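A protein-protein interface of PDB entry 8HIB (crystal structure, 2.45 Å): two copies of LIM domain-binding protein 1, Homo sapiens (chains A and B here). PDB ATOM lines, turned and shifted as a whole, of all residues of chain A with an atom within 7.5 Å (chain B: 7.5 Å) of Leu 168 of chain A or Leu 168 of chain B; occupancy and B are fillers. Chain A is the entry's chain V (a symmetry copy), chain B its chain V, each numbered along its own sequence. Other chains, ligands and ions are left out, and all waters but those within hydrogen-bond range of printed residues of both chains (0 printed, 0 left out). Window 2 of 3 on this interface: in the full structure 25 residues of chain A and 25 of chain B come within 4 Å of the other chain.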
ATOM      1  N   ILE A 157      -1.646   0.117  20.301  1.00  0.00           N
ATOM      2  CA  ILE A 157      -0.926   1.382  20.225  1.00  0.00           C
ATOM      3  C   ILE A 157      -1.701   2.520  20.870  1.00  0.00           C
ATOM      4  O   ILE A 157      -1.122   3.578  21.136  1.00  0.00           O
ATOM      5  CB  ILE A 157      -0.547   1.540  18.737  1.00  0.00           C
ATOM      6  CG1 ILE A 157       0.528   0.495  18.411  1.00  0.00           C
ATOM      7  CG2 ILE A 157      -0.097   2.942  18.398  1.00  0.00           C
ATOM      8  CD1 ILE A 157       1.440   0.830  17.286  1.00  0.00           C
ATOM      9  N   LEU A 158      -2.987   2.332  21.170  1.00  0.00           N
ATOM     10  CA  LEU A 158      -3.627   3.226  22.131  1.00  0.00           C
ATOM     11  C   LEU A 158      -3.122   2.937  23.537  1.00  0.00           C
ATOM     12  O   LEU A 158      -2.799   3.861  24.290  1.00  0.00           O
ATOM     13  CB  LEU A 158      -5.151   3.085  22.080  1.00  0.00           C
ATOM     14  CG  LEU A 158      -6.039   3.819  23.112  1.00  0.00           C
ATOM     15  CD1 LEU A 158      -5.521   5.204  23.454  1.00  0.00           C
ATOM     16  CD2 LEU A 158      -7.506   3.894  22.693  1.00  0.00           C
ATOM     17  N   ALA A 159      -3.039   1.655  23.906  1.00  0.00           N
ATOM     18  CA  ALA A 159      -2.585   1.297  25.245  1.00  0.00           C
ATOM     19  C   ALA A 159      -1.112   1.633  25.452  1.00  0.00           C
ATOM     20  O   ALA A 159      -0.685   1.874  26.585  1.00  0.00           O
ATOM     21  CB  ALA A 159      -2.844  -0.187  25.501  1.00  0.00           C
ATOM     22  N   HIS A 161       0.625   4.412  24.314  1.00  0.00           N
ATOM     23  CA  HIS A 161       0.659   5.825  24.691  1.00  0.00           C
ATOM     24  C   HIS A 161      -0.520   6.197  25.588  1.00  0.00           C
ATOM     25  O   HIS A 161      -1.036   7.318  25.524  1.00  0.00           O
ATOM     26  CB  HIS A 161       0.679   6.693  23.433  1.00  0.00           C
ATOM     27  CG  HIS A 161       1.607   6.207  22.352  1.00  0.00           C
ATOM     28  ND1 HIS A 161       1.698   6.824  21.121  1.00  0.00           N
ATOM     29  CD2 HIS A 161       2.492   5.181  22.317  1.00  0.00           C
ATOM     30  CE1 HIS A 161       2.589   6.197  20.375  1.00  0.00           C
ATOM     31  NE2 HIS A 161       3.082   5.191  21.075  1.00  0.00           N
ATOM     32  N   ALA A 162      -0.954   5.264  26.443  1.00  0.00           N
ATOM     33  CA  ALA A 162      -2.226   5.403  27.146  1.00  0.00           C
ATOM     34  C   ALA A 162      -2.190   6.543  28.155  1.00  0.00           C
ATOM     35  O   ALA A 162      -2.969   7.495  28.060  1.00  0.00           O
ATOM     36  CB  ALA A 162      -2.591   4.085  27.835  1.00  0.00           C
ATOM     37  N   GLN A 163      -1.307   6.453  29.144  1.00  0.00           N
ATOM     38  CA  GLN A 163      -1.154   7.517  30.131  1.00  0.00           C
ATOM     39  C   GLN A 163       0.083   8.344  29.798  1.00  0.00           C
ATOM     40  O   GLN A 163       1.116   8.296  30.465  1.00  0.00           O
ATOM     41  CB  GLN A 163      -1.086   6.940  31.534  1.00  0.00           C
ATOM     42  CG  GLN A 163      -1.245   7.994  32.606  1.00  0.00           C
ATOM     43  CD  GLN A 163      -1.809   7.424  33.880  1.00  0.00           C
ATOM     44  OE1 GLN A 163      -1.287   7.662  34.970  1.00  0.00           O
ATOM     45  NE2 GLN A 163      -2.886   6.655  33.752  1.00  0.00           N
ATOM     46  N   ASP A 164      -0.052   9.109  28.720  1.00  0.00           N
ATOM     47  CA  ASP A 164       1.008  10.000  28.250  1.00  0.00           C
ATOM     48  C   ASP A 164       0.325  11.140  27.517  1.00  0.00           C
ATOM     49  O   ASP A 164       0.221  11.138  26.284  1.00  0.00           O
ATOM     50  CB  ASP A 164       1.993   9.263  27.341  1.00  0.00           C
ATOM     51  CG  ASP A 164       3.117  10.153  26.842  1.00  0.00           C
ATOM     52  OD1 ASP A 164       3.222  11.313  27.297  1.00  0.00           O
ATOM     53  OD2 ASP A 164       3.892   9.697  25.974  1.00  0.00           O
ATOM     54  N   PRO A 165      -0.172  12.139  28.253  1.00  0.00           N
ATOM     55  CA  PRO A 165      -1.083  13.131  27.655  1.00  0.00           C
ATOM     56  C   PRO A 165      -0.600  13.767  26.357  1.00  0.00           C
ATOM     57  O   PRO A 165      -1.439  14.112  25.516  1.00  0.00           O
ATOM     58  CB  PRO A 165      -1.218  14.176  28.770  1.00  0.00           C
ATOM     59  CG  PRO A 165      -1.055  13.387  30.023  1.00  0.00           C
ATOM     60  CD  PRO A 165      -0.035  12.321  29.709  1.00  0.00           C
ATOM     61  N   GLN A 166       0.716  13.930  26.162  1.00  0.00           N
ATOM     62  CA  GLN A 166       1.225  14.616  24.976  1.00  0.00           C
ATOM     63  C   GLN A 166       1.270  13.710  23.747  1.00  0.00           C
ATOM     64  O   GLN A 166       1.139  14.194  22.615  1.00  0.00           O
ATOM     65  CB  GLN A 166       2.613  15.209  25.261  1.00  0.00           C
ATOM     66  CG  GLN A 166       3.690  14.235  25.756  1.00  0.00           C
ATOM     67  CD  GLN A 166       4.267  13.364  24.643  1.00  0.00           C
ATOM     68  OE1 GLN A 166       4.709  13.862  23.605  1.00  0.00           O
ATOM     69  NE2 GLN A 166       4.288  12.056  24.873  1.00  0.00           N
ATOM     70  N   MET A 167       1.457  12.407  23.948  1.00  0.00           N
ATOM     71  CA  MET A 167       1.445  11.457  22.844  1.00  0.00           C
ATOM     72  C   MET A 167       0.024  11.077  22.446  1.00  0.00           C
ATOM     73  O   MET A 167      -0.221  10.737  21.284  1.00  0.00           O
ATOM     74  CB  MET A 167       2.232  10.204  23.235  1.00  0.00           C
ATOM     75  CG  MET A 167       2.904   9.475  22.093  1.00  0.00           C
ATOM     76  SD  MET A 167       3.512  10.530  20.774  1.00  0.00           S
ATOM     77  CE  MET A 167       4.719   9.449  20.007  1.00  0.00           C
ATOM     78  N   LEU A 168      -0.918  11.156  23.390  1.00  0.00           N
ATOM     79  CA  LEU A 168      -2.276  10.683  23.174  1.00  0.00           C
ATOM     80  C   LEU A 168      -3.165  11.718  22.492  1.00  0.00           C
ATOM     81  O   LEU A 168      -4.183  11.344  21.902  1.00  0.00           O
ATOM     82  CB  LEU A 168      -2.879  10.232  24.513  1.00  0.00           C
ATOM     83  CG  LEU A 168      -4.284   9.636  24.492  1.00  0.00           C
ATOM     84  CD1 LEU A 168      -4.306   8.511  23.501  1.00  0.00           C
ATOM     85  CD2 LEU A 168      -4.663   9.121  25.854  1.00  0.00           C
ATOM     86  N   ASP A 169      -2.802  12.997  22.534  1.00  0.00           N
ATOM     87  CA  ASP A 169      -3.488  13.994  21.721  1.00  0.00           C
ATOM     88  C   ASP A 169      -2.836  14.179  20.354  1.00  0.00           C
ATOM     89  O   ASP A 169      -3.435  14.807  19.474  1.00  0.00           O
ATOM     90  CB  ASP A 169      -3.535  15.345  22.434  1.00  0.00           C
ATOM     91  CG  ASP A 169      -2.178  15.985  22.537  1.00  0.00           C
ATOM     92  OD1 ASP A 169      -1.338  15.469  23.296  1.00  0.00           O
ATOM     93  OD2 ASP A 169      -1.946  16.998  21.843  1.00  0.00           O
ATOM     94  N   GLN A 170      -1.616  13.679  20.165  1.00  0.00           N
ATOM     95  CA  GLN A 170      -1.101  13.534  18.814  1.00  0.00           C
ATOM     96  C   GLN A 170      -1.832  12.411  18.086  1.00  0.00           C
ATOM     97  O   GLN A 170      -1.919  12.419  16.853  1.00  0.00           O
ATOM     98  CB  GLN A 170       0.405  13.267  18.852  1.00  0.00           C
ATOM     99  CG  GLN A 170       1.096  13.449  17.501  1.00  0.00           C
ATOM    100  CD  GLN A 170       2.310  12.549  17.320  1.00  0.00           C
ATOM    101  OE1 GLN A 170       2.501  11.585  18.060  1.00  0.00           O
ATOM    102  NE2 GLN A 170       3.140  12.868  16.331  1.00  0.00           N
ATOM    103  N   LEU A 171      -2.374  11.452  18.838  1.00  0.00           N
ATOM    104  CA  LEU A 171      -3.172  10.362  18.298  1.00  0.00           C
ATOM    105  C   LEU A 171      -4.587  10.782  17.944  1.00  0.00           C
ATOM    106  O   LEU A 171      -5.328   9.972  17.385  1.00  0.00           O
ATOM    107  CB  LEU A 171      -3.222   9.201  19.292  1.00  0.00           C
ATOM    108  CG  LEU A 171      -1.927   8.406  19.439  1.00  0.00           C
ATOM    109  CD1 LEU A 171      -2.171   7.140  20.236  1.00  0.00           C
ATOM    110  CD2 LEU A 171      -1.344   8.084  18.071  1.00  0.00           C
ATOM    111  N   SER A 172      -4.990  12.005  18.260  1.00  0.00           N
ATOM    112  CA  SER A 172      -6.278  12.519  17.823  1.00  0.00           C
ATOM    113  C   SER A 172      -6.168  13.366  16.563  1.00  0.00           C
ATOM    114  O   SER A 172      -7.196  13.809  16.041  1.00  0.00           O
ATOM    115  CB  SER A 172      -6.929  13.329  18.940  1.00  0.00           C
ATOM    116  OG  SER A 172      -5.943  14.026  19.674  1.00  0.00           O
ATOM    117  N   LYS A 173      -4.951  13.593  16.067  1.00  0.00           N
ATOM    118  CA  LYS A 173      -4.717  14.333  14.831  1.00  0.00           C
ATOM    119  C   LYS A 173      -4.661  13.365  13.659  1.00  0.00           C
ATOM    120  O   LYS A 173      -3.898  12.394  13.685  1.00  0.00           O
ATOM    121  CB  LYS A 173      -3.405  15.123  14.904  1.00  0.00           C
ATOM    122  CG  LYS A 173      -3.546  16.581  15.330  1.00  0.00           C
ATOM    123  CD  LYS A 173      -2.558  16.948  16.437  1.00  0.00           C
ATOM    124  CE  LYS A 173      -3.116  18.070  17.293  1.00  0.00           C
ATOM    125  NZ  LYS A 173      -2.085  18.750  18.134  1.00  0.00           N
ATOM    126  N   ILE B 157     -13.486   8.297  17.340  1.00  0.00           N
ATOM    127  CA  ILE B 157     -14.018   7.723  18.571  1.00  0.00           C
ATOM    128  C   ILE B 157     -12.959   7.621  19.658  1.00  0.00           C
ATOM    129  O   ILE B 157     -13.303   7.424  20.827  1.00  0.00           O
ATOM    130  CB  ILE B 157     -14.711   6.414  18.137  1.00  0.00           C
ATOM    131  CG1 ILE B 157     -15.970   6.789  17.343  1.00  0.00           C
ATOM    132  CG2 ILE B 157     -15.026   5.508  19.305  1.00  0.00           C
ATOM    133  CD1 ILE B 157     -17.065   5.783  17.350  1.00  0.00           C
ATOM    134  N   LEU B 158     -11.679   7.790  19.324  1.00  0.00           N
ATOM    135  CA  LEU B 158     -10.710   8.099  20.371  1.00  0.00           C
ATOM    136  C   LEU B 158     -10.904   9.527  20.864  1.00  0.00           C
ATOM    137  O   LEU B 158     -10.905   9.778  22.074  1.00  0.00           O
ATOM    138  CB  LEU B 158      -9.276   7.907  19.867  1.00  0.00           C
ATOM    139  CG  LEU B 158      -8.075   8.321  20.749  1.00  0.00           C
ATOM    140  CD1 LEU B 158      -8.296   8.021  22.221  1.00  0.00           C
ATOM    141  CD2 LEU B 158      -6.753   7.714  20.281  1.00  0.00           C
ATOM    142  N   ALA B 159     -11.078  10.475  19.940  1.00  0.00           N
ATOM    143  CA  ALA B 159     -11.248  11.870  20.331  1.00  0.00           C
ATOM    144  C   ALA B 159     -12.568  12.095  21.062  1.00  0.00           C
ATOM    145  O   ALA B 159     -12.677  13.018  21.873  1.00  0.00           O
ATOM    146  CB  ALA B 159     -11.150  12.769  19.100  1.00  0.00           C
ATOM    147  N   HIS B 161     -14.113  10.017  23.370  1.00  0.00           N
ATOM    148  CA  HIS B 161     -13.857   9.667  24.767  1.00  0.00           C
ATOM    149  C   HIS B 161     -12.459  10.096  25.207  1.00  0.00           C
ATOM    150  O   HIS B 161     -11.819   9.427  26.026  1.00  0.00           O
ATOM    151  CB  HIS B 161     -14.051   8.164  24.965  1.00  0.00           C
ATOM    152  CG  HIS B 161     -15.266   7.594  24.284  1.00  0.00           C
ATOM    153  ND1 HIS B 161     -15.557   6.246  24.293  1.00  0.00           N
ATOM    154  CD2 HIS B 161     -16.271   8.184  23.590  1.00  0.00           C
ATOM    155  CE1 HIS B 161     -16.680   6.029  23.631  1.00  0.00           C
ATOM    156  NE2 HIS B 161     -17.130   7.189  23.188  1.00  0.00           N
ATOM    157  N   ALA B 162     -11.972  11.224  24.677  1.00  0.00           N
ATOM    158  CA  ALA B 162     -10.563  11.584  24.808  1.00  0.00           C
ATOM    159  C   ALA B 162     -10.198  11.912  26.250  1.00  0.00           C
ATOM    160  O   ALA B 162      -9.336  11.261  26.847  1.00  0.00           O
ATOM    161  CB  ALA B 162     -10.236  12.763  23.888  1.00  0.00           C
ATOM    162  N   GLN B 163     -10.826  12.936  26.819  1.00  0.00           N
ATOM    163  CA  GLN B 163     -10.588  13.298  28.213  1.00  0.00           C
ATOM    164  C   GLN B 163     -11.739  12.786  29.073  1.00  0.00           C
ATOM    165  O   GLN B 163     -12.581  13.532  29.571  1.00  0.00           O
ATOM    166  CB  GLN B 163     -10.404  14.799  28.352  1.00  0.00           C
ATOM    167  CG  GLN B 163      -9.849  15.196  29.702  1.00  0.00           C
ATOM    168  CD  GLN B 163      -9.086  16.492  29.640  1.00  0.00           C
ATOM    169  OE1 GLN B 163      -9.296  17.393  30.452  1.00  0.00           O
ATOM    170  NE2 GLN B 163      -8.190  16.599  28.663  1.00  0.00           N
ATOM    171  N   ASP B 164     -11.756  11.467  29.224  1.00  0.00           N
ATOM    172  CA  ASP B 164     -12.760  10.781  30.038  1.00  0.00           C
ATOM    173  C   ASP B 164     -12.115   9.501  30.536  1.00  0.00           C
ATOM    174  O   ASP B 164     -12.307   8.422  29.963  1.00  0.00           O
ATOM    175  CB  ASP B 164     -14.026  10.490  29.230  1.00  0.00           C
ATOM    176  CG  ASP B 164     -15.098   9.788  30.044  1.00  0.00           C
ATOM    177  OD1 ASP B 164     -14.928   9.638  31.273  1.00  0.00           O
ATOM    178  OD2 ASP B 164     -16.113   9.368  29.448  1.00  0.00           O
ATOM    179  N   PRO B 165     -11.321   9.586  31.608  1.00  0.00           N
ATOM    180  CA  PRO B 165     -10.447   8.460  31.986  1.00  0.00           C
ATOM    181  C   PRO B 165     -11.129   7.100  32.075  1.00  0.00           C
ATOM    182  O   PRO B 165     -10.471   6.089  31.801  1.00  0.00           O
ATOM    183  CB  PRO B 165      -9.905   8.903  33.352  1.00  0.00           C
ATOM    184  CG  PRO B 165      -9.878  10.389  33.264  1.00  0.00           C
ATOM    185  CD  PRO B 165     -11.083  10.777  32.445  1.00  0.00           C
ATOM    186  N   GLN B 166     -12.416   7.040  32.440  1.00  0.00           N
ATOM    187  CA  GLN B 166     -13.088   5.755  32.628  1.00  0.00           C
ATOM    188  C   GLN B 166     -13.551   5.136  31.311  1.00  0.00           C
ATOM    189  O   GLN B 166     -13.624   3.906  31.196  1.00  0.00           O
ATOM    190  CB  GLN B 166     -14.271   5.913  33.594  1.00  0.00           C
ATOM    191  CG  GLN B 166     -15.328   6.963  33.227  1.00  0.00           C
ATOM    192  CD  GLN B 166     -16.268   6.502  32.117  1.00  0.00           C
ATOM    193  OE1 GLN B 166     -16.868   5.427  32.191  1.00  0.00           O
ATOM    194  NE2 GLN B 166     -16.420   7.334  31.093  1.00  0.00           N
ATOM    195  N   MET B 167     -13.868   5.965  30.317  1.00  0.00           N
ATOM    196  CA  MET B 167     -14.252   5.467  29.003  1.00  0.00           C
ATOM    197  C   MET B 167     -13.033   5.104  28.163  1.00  0.00           C
ATOM    198  O   MET B 167     -13.120   4.229  27.296  1.00  0.00           O
ATOM    199  CB  MET B 167     -15.093   6.520  28.279  1.00  0.00           C
ATOM    200  CG  MET B 167     -16.112   5.980  27.302  1.00  0.00           C
ATOM    201  SD  MET B 167     -16.859   4.416  27.772  1.00  0.00           S
ATOM    202  CE  MET B 167     -18.354   4.444  26.783  1.00  0.00           C
ATOM    203  N   LEU B 168     -11.893   5.748  28.426  1.00  0.00           N
ATOM    204  CA  LEU B 168     -10.705   5.598  27.600  1.00  0.00           C
ATOM    205  C   LEU B 168      -9.866   4.383  27.983  1.00  0.00           C
ATOM    206  O   LEU B 168      -9.080   3.909  27.157  1.00  0.00           O
ATOM    207  CB  LEU B 168      -9.874   6.887  27.662  1.00  0.00           C
ATOM    208  CG  LEU B 168      -8.612   6.958  26.805  1.00  0.00           C
ATOM    209  CD1 LEU B 168      -8.985   6.640  25.388  1.00  0.00           C
ATOM    210  CD2 LEU B 168      -7.999   8.331  26.874  1.00  0.00           C
ATOM    211  N   ASP B 169     -10.024   3.855  29.194  1.00  0.00           N
ATOM    212  CA  ASP B 169      -9.416   2.574  29.532  1.00  0.00           C
ATOM    213  C   ASP B 169     -10.339   1.395  29.240  1.00  0.00           C
ATOM    214  O   ASP B 169      -9.882   0.246  29.251  1.00  0.00           O
ATOM    215  CB  ASP B 169      -9.011   2.533  31.006  1.00  0.00           C
ATOM    216  CG  ASP B 169     -10.200   2.505  31.927  1.00  0.00           C
ATOM    217  OD1 ASP B 169     -10.901   3.529  32.015  1.00  0.00           O
ATOM    218  OD2 ASP B 169     -10.443   1.450  32.549  1.00  0.00           O
ATOM    219  N   GLN B 170     -11.627   1.645  29.013  1.00  0.00           N
ATOM    220  CA  GLN B 170     -12.462   0.621  28.411  1.00  0.00           C
ATOM    221  C   GLN B 170     -12.091   0.428  26.945  1.00  0.00           C
ATOM    222  O   GLN B 170     -12.297  -0.654  26.384  1.00  0.00           O
ATOM    223  CB  GLN B 170     -13.939   0.995  28.553  1.00  0.00           C
ATOM    224  CG  GLN B 170     -14.897  -0.163  28.274  1.00  0.00           C
ATOM    225  CD  GLN B 170     -16.234   0.286  27.703  1.00  0.00           C
ATOM    226  OE1 GLN B 170     -16.379   1.418  27.242  1.00  0.00           O
ATOM    227  NE2 GLN B 170     -17.220  -0.605  27.736  1.00  0.00           N
ATOM    228  N   LEU B 171     -11.528   1.465  26.320  1.00  0.00           N
ATOM    229  CA  LEU B 171     -11.043   1.410  24.949  1.00  0.00           C
ATOM    230  C   LEU B 171      -9.706   0.701  24.821  1.00  0.00           C
ATOM    231  O   LEU B 171      -9.241   0.504  23.698  1.00  0.00           O
ATOM    232  CB  LEU B 171     -10.924   2.821  24.374  1.00  0.00           C
ATOM    233  CG  LEU B 171     -12.247   3.515  24.059  1.00  0.00           C
ATOM    234  CD1 LEU B 171     -12.003   4.780  23.259  1.00  0.00           C
ATOM    235  CD2 LEU B 171     -13.176   2.570  23.311  1.00  0.00           C
ATOM    236  N   SER B 172      -9.072   0.327  25.924  1.00  0.00           N
ATOM    237  CA  SER B 172      -7.863  -0.480  25.870  1.00  0.00           C
ATOM    238  C   SER B 172      -8.147  -1.962  26.069  1.00  0.00           C
ATOM    239  O   SER B 172      -7.220  -2.773  25.978  1.00  0.00           O
ATOM    240  CB  SER B 172      -6.859   0.003  26.912  1.00  0.00           C
ATOM    241  OG  SER B 172      -7.535   0.441  28.073  1.00  0.00           O
ATOM    242  N   LYS B 173      -9.402  -2.329  26.334  1.00  0.00           N
ATOM    243  CA  LYS B 173      -9.814  -3.721  26.481  1.00  0.00           C
ATOM    244  C   LYS B 173     -10.282  -4.260  25.137  1.00  0.00           C
ATOM    245  O   LYS B 173     -11.148  -3.661  24.489  1.00  0.00           O
ATOM    246  CB  LYS B 173     -10.946  -3.853  27.507  1.00  0.00           C
ATOM    247  CG  LYS B 173     -10.504  -4.207  28.923  1.00  0.00           C
ATOM    248  CD  LYS B 173     -11.141  -3.287  29.963  1.00  0.00           C
ATOM    249  CE  LYS B 173     -10.242  -3.166  31.181  1.00  0.00           C
ATOM    250  NZ  LYS B 173     -10.939  -2.622  32.386  1.00  0.00           N
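Leu 158 of chain A touches Leu 171 of chain B, and with the chains exchanged Leu 171 of chain A touches Leu 158 of chain B.
Leu 168 of chain B touches its own counterpart, Leu 168 of chain A.
Positions printed for both chains: 157, 158, 159, 161, 162, 163, 164, 165, 166, 167, 168, 169, 170, 171, 172 and 173.
Of the 3 pairs that touch across the chains among the printed residues, 3 have their exchanged pair printed and touching as well.
Of the 16 printed residues of chain B, 3 touch a printed residue of chain A.
Printed residues of chain A that touch a printed residue of chain B: Leu 158, Leu 168 and Leu 171.
Hydrophobic or aromatic side chains of chain A within 4 Å of the printed part of chain B: Leu 158, Leu 168 and Leu 171.
Among the printed residues, 3 pairs touch across the chains.
Among the printed residues, no Asp or Glu carboxylate lies within 4 Å of a Lys or Arg side-chain nitrogen of the other chain.
Among the printed residues, merely in contact across the chains: Leu 168 of chain A with Leu 168 of chain B (3.6 Å), Leu 158 of chain A with Leu 171 of chain B (3.9 Å) and Leu 171 of chain A with Leu 158 of chain B (3.9 Å).
Leu 168 of chain A touches just one residue of chain B: Leu 168.
Printed residues of chain A within 4 Å of Leu 171 of chain B: Leu 158.
Of the printed residues of chain A, Leu 158 of chain B touches Leu 171 (3.9 Å).
Of the printed residues of chain B, Leu 171 of chain A touches Leu 158.
Of the printed residues of chain B, Leu 158 of chain A touches Leu 171.
Gln 163 of chain A touches none of the printed residues of chain B.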
